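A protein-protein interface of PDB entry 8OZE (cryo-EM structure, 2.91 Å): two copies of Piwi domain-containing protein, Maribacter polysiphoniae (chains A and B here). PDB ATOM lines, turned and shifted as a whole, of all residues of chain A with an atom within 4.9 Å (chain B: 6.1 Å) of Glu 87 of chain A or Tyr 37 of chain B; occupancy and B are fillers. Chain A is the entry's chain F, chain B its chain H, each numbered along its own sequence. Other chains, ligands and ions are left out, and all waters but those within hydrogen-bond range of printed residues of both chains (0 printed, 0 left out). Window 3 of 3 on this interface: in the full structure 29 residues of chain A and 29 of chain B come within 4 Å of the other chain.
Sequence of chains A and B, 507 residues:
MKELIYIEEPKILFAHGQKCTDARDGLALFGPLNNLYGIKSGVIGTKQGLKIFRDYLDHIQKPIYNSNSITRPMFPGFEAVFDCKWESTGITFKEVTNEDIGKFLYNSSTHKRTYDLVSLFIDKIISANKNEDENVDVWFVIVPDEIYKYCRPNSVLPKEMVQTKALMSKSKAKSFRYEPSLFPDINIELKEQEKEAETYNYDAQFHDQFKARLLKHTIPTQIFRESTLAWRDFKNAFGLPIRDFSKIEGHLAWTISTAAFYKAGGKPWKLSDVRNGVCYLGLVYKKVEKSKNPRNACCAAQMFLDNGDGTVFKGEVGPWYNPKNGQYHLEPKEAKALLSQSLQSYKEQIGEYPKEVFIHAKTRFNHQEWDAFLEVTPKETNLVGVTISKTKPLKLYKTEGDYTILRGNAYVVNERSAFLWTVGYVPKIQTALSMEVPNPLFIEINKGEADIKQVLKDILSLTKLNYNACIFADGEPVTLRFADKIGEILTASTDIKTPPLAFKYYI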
ATOM      1  N   TYR A  37     -16.400  19.244 -14.304  1.00  0.00           N
ATOM      2  CA  TYR A  37     -17.134  20.494 -14.153  1.00  0.00           C
ATOM      3  C   TYR A  37     -16.856  21.151 -12.810  1.00  0.00           C
ATOM      4  O   TYR A  37     -16.871  22.382 -12.708  1.00  0.00           O
ATOM      5  CB  TYR A  37     -18.628  20.245 -14.332  1.00  0.00           C
ATOM      6  CG  TYR A  37     -18.964  19.472 -15.582  1.00  0.00           C
ATOM      7  CD1 TYR A  37     -18.924  20.081 -16.824  1.00  0.00           C
ATOM      8  CD2 TYR A  37     -19.312  18.133 -15.519  1.00  0.00           C
ATOM      9  CE1 TYR A  37     -19.229  19.379 -17.970  1.00  0.00           C
ATOM     10  CE2 TYR A  37     -19.618  17.423 -16.659  1.00  0.00           C
ATOM     11  CZ  TYR A  37     -19.575  18.051 -17.882  1.00  0.00           C
ATOM     12  OH  TYR A  37     -19.879  17.347 -19.024  1.00  0.00           O
ATOM     13  N   GLY A  38     -16.601  20.360 -11.778  1.00  0.00           N
ATOM     14  CA  GLY A  38     -16.291  20.916 -10.478  1.00  0.00           C
ATOM     15  C   GLY A  38     -15.925  19.829  -9.497  1.00  0.00           C
ATOM     16  O   GLY A  38     -16.273  18.659  -9.676  1.00  0.00           O
ATOM     17  N   ILE A  39     -15.215  20.237  -8.451  1.00  0.00           N
ATOM     18  CA  ILE A  39     -14.813  19.346  -7.371  1.00  0.00           C
ATOM     19  C   ILE A  39     -15.584  19.759  -6.128  1.00  0.00           C
ATOM     20  O   ILE A  39     -15.381  20.856  -5.595  1.00  0.00           O
ATOM     21  CB  ILE A  39     -13.302  19.386  -7.120  1.00  0.00           C
ATOM     22  CG1 ILE A  39     -12.545  18.903  -8.355  1.00  0.00           C
ATOM     23  CG2 ILE A  39     -12.942  18.533  -5.915  1.00  0.00           C
ATOM     24  CD1 ILE A  39     -11.051  18.955  -8.201  1.00  0.00           C
ATOM     25  N   LYS A  40     -16.472  18.883  -5.667  1.00  0.00           N
ATOM     26  CA  LYS A  40     -17.231  19.108  -4.443  1.00  0.00           C
ATOM     27  C   LYS A  40     -16.446  18.490  -3.294  1.00  0.00           C
ATOM     28  O   LYS A  40     -16.252  17.272  -3.250  1.00  0.00           O
ATOM     29  CB  LYS A  40     -18.626  18.504  -4.562  1.00  0.00           C
ATOM     30  CG  LYS A  40     -19.311  18.826  -5.874  1.00  0.00           C
ATOM     31  CD  LYS A  40     -20.518  17.940  -6.104  1.00  0.00           C
ATOM     32  CE  LYS A  40     -20.972  18.003  -7.551  1.00  0.00           C
ATOM     33  NZ  LYS A  40     -22.095  17.061  -7.816  1.00  0.00           N
ATOM     34  N   SER A  41     -15.992  19.327  -2.369  1.00  0.00           N
ATOM     35  CA  SER A  41     -15.034  18.915  -1.354  1.00  0.00           C
ATOM     36  C   SER A  41     -15.715  18.743  -0.005  1.00  0.00           C
ATOM     37  O   SER A  41     -16.466  19.618   0.439  1.00  0.00           O
ATOM     38  CB  SER A  41     -13.896  19.929  -1.244  1.00  0.00           C
ATOM     39  OG  SER A  41     -14.395  21.247  -1.162  1.00  0.00           O
ATOM     40  N   LEU A  57      -7.443  27.251   0.669  1.00  0.00           N
ATOM     41  CA  LEU A  57      -8.095  27.062  -0.619  1.00  0.00           C
ATOM     42  C   LEU A  57      -8.348  28.407  -1.286  1.00  0.00           C
ATOM     43  O   LEU A  57      -8.205  28.540  -2.508  1.00  0.00           O
ATOM     44  CB  LEU A  57      -9.385  26.264  -0.437  1.00  0.00           C
ATOM     45  CG  LEU A  57     -10.027  25.663  -1.689  1.00  0.00           C
ATOM     46  CD1 LEU A  57     -10.786  24.408  -1.310  1.00  0.00           C
ATOM     47  CD2 LEU A  57     -10.948  26.639  -2.393  1.00  0.00           C
ATOM     48  N   GLN A  61      -6.774  29.700  -4.819  1.00  0.00           N
ATOM     49  CA  GLN A  61      -7.678  30.209  -5.846  1.00  0.00           C
ATOM     50  C   GLN A  61      -6.969  31.197  -6.764  1.00  0.00           C
ATOM     51  O   GLN A  61      -7.175  31.181  -7.983  1.00  0.00           O
ATOM     52  CB  GLN A  61      -8.900  30.865  -5.205  1.00  0.00           C
ATOM     53  CG  GLN A  61      -9.955  29.885  -4.727  1.00  0.00           C
ATOM     54  CD  GLN A  61     -10.154  28.730  -5.683  1.00  0.00           C
ATOM     55  OE1 GLN A  61      -9.891  27.579  -5.342  1.00  0.00           O
ATOM     56  NE2 GLN A  61     -10.623  29.031  -6.889  1.00  0.00           N
ATOM     57  N   LYS A  85     -13.970  23.877 -11.344  1.00  0.00           N
ATOM     58  CA  LYS A  85     -14.392  24.761 -10.265  1.00  0.00           C
ATOM     59  C   LYS A  85     -14.219  24.041  -8.932  1.00  0.00           C
ATOM     60  O   LYS A  85     -15.009  23.158  -8.587  1.00  0.00           O
ATOM     61  CB  LYS A  85     -15.836  25.206 -10.471  1.00  0.00           C
ATOM     62  CG  LYS A  85     -15.968  26.589 -11.086  1.00  0.00           C
ATOM     63  CD  LYS A  85     -17.348  26.815 -11.675  1.00  0.00           C
ATOM     64  CE  LYS A  85     -17.463  26.207 -13.061  1.00  0.00           C
ATOM     65  NZ  LYS A  85     -18.848  26.312 -13.596  1.00  0.00           N
ATOM     66  N   TRP A  86     -13.185  24.421  -8.183  1.00  0.00           N
ATOM     67  CA  TRP A  86     -12.940  23.905  -6.836  1.00  0.00           C
ATOM     68  C   TRP A  86     -12.961  25.103  -5.892  1.00  0.00           C
ATOM     69  O   TRP A  86     -11.916  25.675  -5.573  1.00  0.00           O
ATOM     70  CB  TRP A  86     -11.623  23.147  -6.757  1.00  0.00           C
ATOM     71  CG  TRP A  86     -11.429  22.433  -5.460  1.00  0.00           C
ATOM     72  CD1 TRP A  86     -12.397  21.886  -4.675  1.00  0.00           C
ATOM     73  CD2 TRP A  86     -10.189  22.206  -4.784  1.00  0.00           C
ATOM     74  NE1 TRP A  86     -11.837  21.323  -3.556  1.00  0.00           N
ATOM     75  CE2 TRP A  86     -10.481  21.508  -3.600  1.00  0.00           C
ATOM     76  CE3 TRP A  86      -8.858  22.522  -5.067  1.00  0.00           C
ATOM     77  CZ2 TRP A  86      -9.494  21.125  -2.699  1.00  0.00           C
ATOM     78  CZ3 TRP A  86      -7.880  22.136  -4.172  1.00  0.00           C
ATOM     79  CH2 TRP A  86      -8.202  21.445  -3.004  1.00  0.00           C
ATOM     80  N   GLU A  87     -14.152  25.472  -5.438  1.00  0.00           N
ATOM     81  CA  GLU A  87     -14.350  26.660  -4.625  1.00  0.00           C
ATOM     82  C   GLU A  87     -14.298  26.317  -3.142  1.00  0.00           C
ATOM     83  O   GLU A  87     -14.317  25.153  -2.738  1.00  0.00           O
ATOM     84  CB  GLU A  87     -15.689  27.324  -4.964  1.00  0.00           C
ATOM     85  CG  GLU A  87     -16.009  27.381  -6.447  1.00  0.00           C
ATOM     86  CD  GLU A  87     -14.894  28.003  -7.262  1.00  0.00           C
ATOM     87  OE1 GLU A  87     -14.355  29.045  -6.836  1.00  0.00           O
ATOM     88  OE2 GLU A  87     -14.555  27.451  -8.328  1.00  0.00           O
ATOM     89  N   SER A  88     -14.223  27.365  -2.325  1.00  0.00           N
ATOM     90  CA  SER A  88     -14.372  27.239  -0.883  1.00  0.00           C
ATOM     91  C   SER A  88     -15.829  27.246  -0.448  1.00  0.00           C
ATOM     92  O   SER A  88     -16.116  26.939   0.714  1.00  0.00           O
ATOM     93  CB  SER A  88     -13.624  28.370  -0.173  1.00  0.00           C
ATOM     94  OG  SER A  88     -13.853  28.333   1.223  1.00  0.00           O
ATOM     95  N   THR A  89     -16.746  27.592  -1.345  1.00  0.00           N
ATOM     96  CA  THR A  89     -18.174  27.542  -1.076  1.00  0.00           C
ATOM     97  C   THR A  89     -18.733  26.252  -1.655  1.00  0.00           C
ATOM     98  O   THR A  89     -18.450  25.910  -2.807  1.00  0.00           O
ATOM     99  CB  THR A  89     -18.895  28.748  -1.679  1.00  0.00           C
ATOM    100  OG1 THR A  89     -18.718  28.750  -3.101  1.00  0.00           O
ATOM    101  CG2 THR A  89     -18.339  30.042  -1.104  1.00  0.00           C
ATOM    102  N   ILE A  91     -18.347  23.339   0.307  1.00  0.00           N
ATOM    103  CA  ILE A  91     -17.656  22.265   1.007  1.00  0.00           C
ATOM    104  C   ILE A  91     -18.561  21.749   2.117  1.00  0.00           C
ATOM    105  O   ILE A  91     -19.277  22.524   2.764  1.00  0.00           O
ATOM    106  CB  ILE A  91     -16.300  22.750   1.546  1.00  0.00           C
ATOM    107  CG1 ILE A  91     -16.452  23.524   2.849  1.00  0.00           C
ATOM    108  CG2 ILE A  91     -15.626  23.654   0.531  1.00  0.00           C
ATOM    109  CD1 ILE A  91     -15.135  23.879   3.480  1.00  0.00           C
ATOM    110  N   ASN B  35     -25.604  24.545  -5.583  1.00  0.00           N
ATOM    111  CA  ASN B  35     -24.850  24.665  -6.827  1.00  0.00           C
ATOM    112  C   ASN B  35     -24.103  23.361  -7.082  1.00  0.00           C
ATOM    113  O   ASN B  35     -23.124  23.050  -6.396  1.00  0.00           O
ATOM    114  CB  ASN B  35     -23.890  25.848  -6.757  1.00  0.00           C
ATOM    115  CG  ASN B  35     -23.188  26.108  -8.073  1.00  0.00           C
ATOM    116  OD1 ASN B  35     -23.620  25.637  -9.125  1.00  0.00           O
ATOM    117  ND2 ASN B  35     -22.097  26.861  -8.023  1.00  0.00           N
ATOM    118  N   LEU B  36     -24.569  22.599  -8.065  1.00  0.00           N
ATOM    119  CA  LEU B  36     -23.833  21.459  -8.599  1.00  0.00           C
ATOM    120  C   LEU B  36     -23.135  21.927  -9.867  1.00  0.00           C
ATOM    121  O   LEU B  36     -23.791  22.348 -10.824  1.00  0.00           O
ATOM    122  CB  LEU B  36     -24.761  20.283  -8.892  1.00  0.00           C
ATOM    123  CG  LEU B  36     -25.393  19.551  -7.715  1.00  0.00           C
ATOM    124  CD1 LEU B  36     -26.064  18.287  -8.208  1.00  0.00           C
ATOM    125  CD2 LEU B  36     -24.349  19.230  -6.666  1.00  0.00           C
ATOM    126  N   TYR B  37     -21.803  21.859  -9.874  1.00  0.00           N
ATOM    127  CA  TYR B  37     -21.057  22.338 -11.031  1.00  0.00           C
ATOM    128  C   TYR B  37     -21.336  21.496 -12.266  1.00  0.00           C
ATOM    129  O   TYR B  37     -21.311  22.014 -13.387  1.00  0.00           O
ATOM    130  CB  TYR B  37     -19.565  22.356 -10.719  1.00  0.00           C
ATOM    131  CG  TYR B  37     -19.229  23.059  -9.428  1.00  0.00           C
ATOM    132  CD1 TYR B  37     -19.257  24.440  -9.344  1.00  0.00           C
ATOM    133  CD2 TYR B  37     -18.894  22.342  -8.292  1.00  0.00           C
ATOM    134  CE1 TYR B  37     -18.952  25.089  -8.168  1.00  0.00           C
ATOM    135  CE2 TYR B  37     -18.588  22.981  -7.111  1.00  0.00           C
ATOM    136  CZ  TYR B  37     -18.618  24.354  -7.054  1.00  0.00           C
ATOM    137  OH  TYR B  37     -18.316  24.999  -5.877  1.00  0.00           O
ATOM    138  N   GLY B  38     -21.604  20.210 -12.088  1.00  0.00           N
ATOM    139  CA  GLY B  38     -21.916  19.356 -13.216  1.00  0.00           C
ATOM    140  C   GLY B  38     -22.299  17.971 -12.756  1.00  0.00           C
ATOM    141  O   GLY B  38     -21.961  17.546 -11.647  1.00  0.00           O
ATOM    142  N   ILE B  39     -23.010  17.268 -13.630  1.00  0.00           N
ATOM    143  CA  ILE B  39     -23.426  15.893 -13.389  1.00  0.00           C
ATOM    144  C   ILE B  39     -22.658  15.008 -14.357  1.00  0.00           C
ATOM    145  O   ILE B  39     -22.853  15.087 -15.575  1.00  0.00           O
ATOM    146  CB  ILE B  39     -24.938  15.710 -13.557  1.00  0.00           C
ATOM    147  CG1 ILE B  39     -25.692  16.552 -12.531  1.00  0.00           C
ATOM    148  CG2 ILE B  39     -25.313  14.243 -13.410  1.00  0.00           C
ATOM    149  CD1 ILE B  39     -27.187  16.459 -12.661  1.00  0.00           C
ATOM    150  N   ASP B  83     -29.031  25.135 -13.492  1.00  0.00           N
ATOM    151  CA  ASP B  83     -27.729  25.797 -13.618  1.00  0.00           C
ATOM    152  C   ASP B  83     -26.567  24.833 -13.398  1.00  0.00           C
ATOM    153  O   ASP B  83     -25.559  25.175 -12.773  1.00  0.00           O
ATOM    154  CB  ASP B  83     -27.645  27.045 -12.712  1.00  0.00           C
ATOM    155  CG  ASP B  83     -27.517  26.739 -11.217  1.00  0.00           C
ATOM    156  OD1 ASP B  83     -27.380  25.578 -10.796  1.00  0.00           O
ATOM    157  OD2 ASP B  83     -27.553  27.712 -10.434  1.00  0.00           O
ATOM    158  N   CYS B  84     -26.701  23.630 -13.948  1.00  0.00           N
ATOM    159  CA  CYS B  84     -25.749  22.546 -13.773  1.00  0.00           C
ATOM    160  C   CYS B  84     -25.467  21.924 -15.130  1.00  0.00           C
ATOM    161  O   CYS B  84     -26.380  21.752 -15.943  1.00  0.00           O
ATOM    162  CB  CYS B  84     -26.296  21.496 -12.801  1.00  0.00           C
ATOM    163  SG  CYS B  84     -25.265  20.049 -12.579  1.00  0.00           S
ATOM    164  N   LYS B  85     -24.205  21.593 -15.377  1.00  0.00           N
ATOM    165  CA  LYS B  85     -23.780  21.084 -16.675  1.00  0.00           C
ATOM    166  C   LYS B  85     -23.967  19.572 -16.708  1.00  0.00           C
ATOM    167  O   LYS B  85     -23.188  18.829 -16.105  1.00  0.00           O
ATOM    168  CB  LYS B  85     -22.330  21.471 -16.954  1.00  0.00           C
ATOM    169  CG  LYS B  85     -22.183  22.686 -17.852  1.00  0.00           C
ATOM    170  CD  LYS B  85     -20.797  23.296 -17.750  1.00  0.00           C
ATOM    171  CE  LYS B  85     -20.680  24.202 -16.539  1.00  0.00           C
ATOM    172  NZ  LYS B  85     -19.292  24.706 -16.357  1.00  0.00           N
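Among the printed residues, merely in contact across the chains: Lys 40 of chain A with Leu 36 of chain B, Tyr 37 of chain A with Tyr 37 of chain B, Glu 87 of chain A with Tyr 37 of chain B, Tyr 37 of chain A with Gly 38 of chain B, Gly 38 of chain A with Tyr 37 of chain B, Tyr 37 of chain A with Lys 85 of chain B, Lys 85 of chain A with Tyr 37 of chain B and Lys 40 of chain A with Gly 38 of chain B.
The backbone NH (N) of Ile 39 of chain B is in hydrogen-bond range of the backbone carbonyl oxygen (O) of Lys 85 of chain B (2.9 Å).
The backbone carbonyl oxygen (O) of Lys 85 of chain A is in hydrogen-bond range of the backbone NH (N) of Ile 39 of chain A, 2.9 Å away.
N of Gly 38 of chain B lies close to SG of Cys 84 of chain B (3.7 Å).
The backbone carbonyl oxygen of Leu 36 of chain B is in hydrogen-bond range of the side-chain sulfur of Cys 84 of chain B (3.2 Å).
Printed residues of chain A that touch a printed residue of chain B: Tyr 37, Gly 38, Lys 40, Lys 85, Glu 87 and Thr 89.
Hydrophobic or aromatic side chains of chain A within 4 Å of the printed part of chain B: Tyr 37.
Among the printed residues, 10 pairs touch across the chains.
Among the printed residues, no Asp or Glu carboxylate lies within 4 Å of a Lys or Arg side-chain nitrogen of the other chain.
Tyr 37 of chain B touches its own counterpart, Tyr 37 of chain A.
Tyr 37 of chain A touches Gly 38 of chain B, and with the chains exchanged Gly 38 of chain A touches Tyr 37 of chain B.
Tyr 37 of chain A touches Lys 85 of chain B, and with the chains exchanged Lys 85 of chain A touches Tyr 37 of chain B.
Lys 85 of chain B touches its own counterpart, Lys 85 of chain A.
Positions printed for both chains: 37, 38, 39 and 85.
NZ of Lys 85 of chain A lies close to NZ of Lys 85 of chain B.
The side-chain hydroxyl (OH) of Tyr 37 of chain B lies within hydrogen-bond range of the backbone carbonyl oxygen (O) of Thr 89 of chain A, 3.2 Å away.
Glu 87 of chain A touches one residue of chain B.
Tyr 37 of chain B touches five residues of chain A.
Printed residues of chain B within 4 Å of Lys 40 of chain A: Leu 36 and Gly 38.
Of the printed residues of chain B, Lys 85 of chain A touches Tyr 37 (3.7 Å) and Lys 85 (3.2 Å).
Ile 91 of chain A touches none of the printed residues of chain B.
Ile 39 of chain A touches none of the printed residues of chain B.
The nearest printed residue of chain B that does not touch Glu 87 of chain A is Asn 35 of chain B (6.3 Å).
The nearest residue of chain A that does not touch Tyr 37 of chain B is Ile 39 of chain A (4.1 Å).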
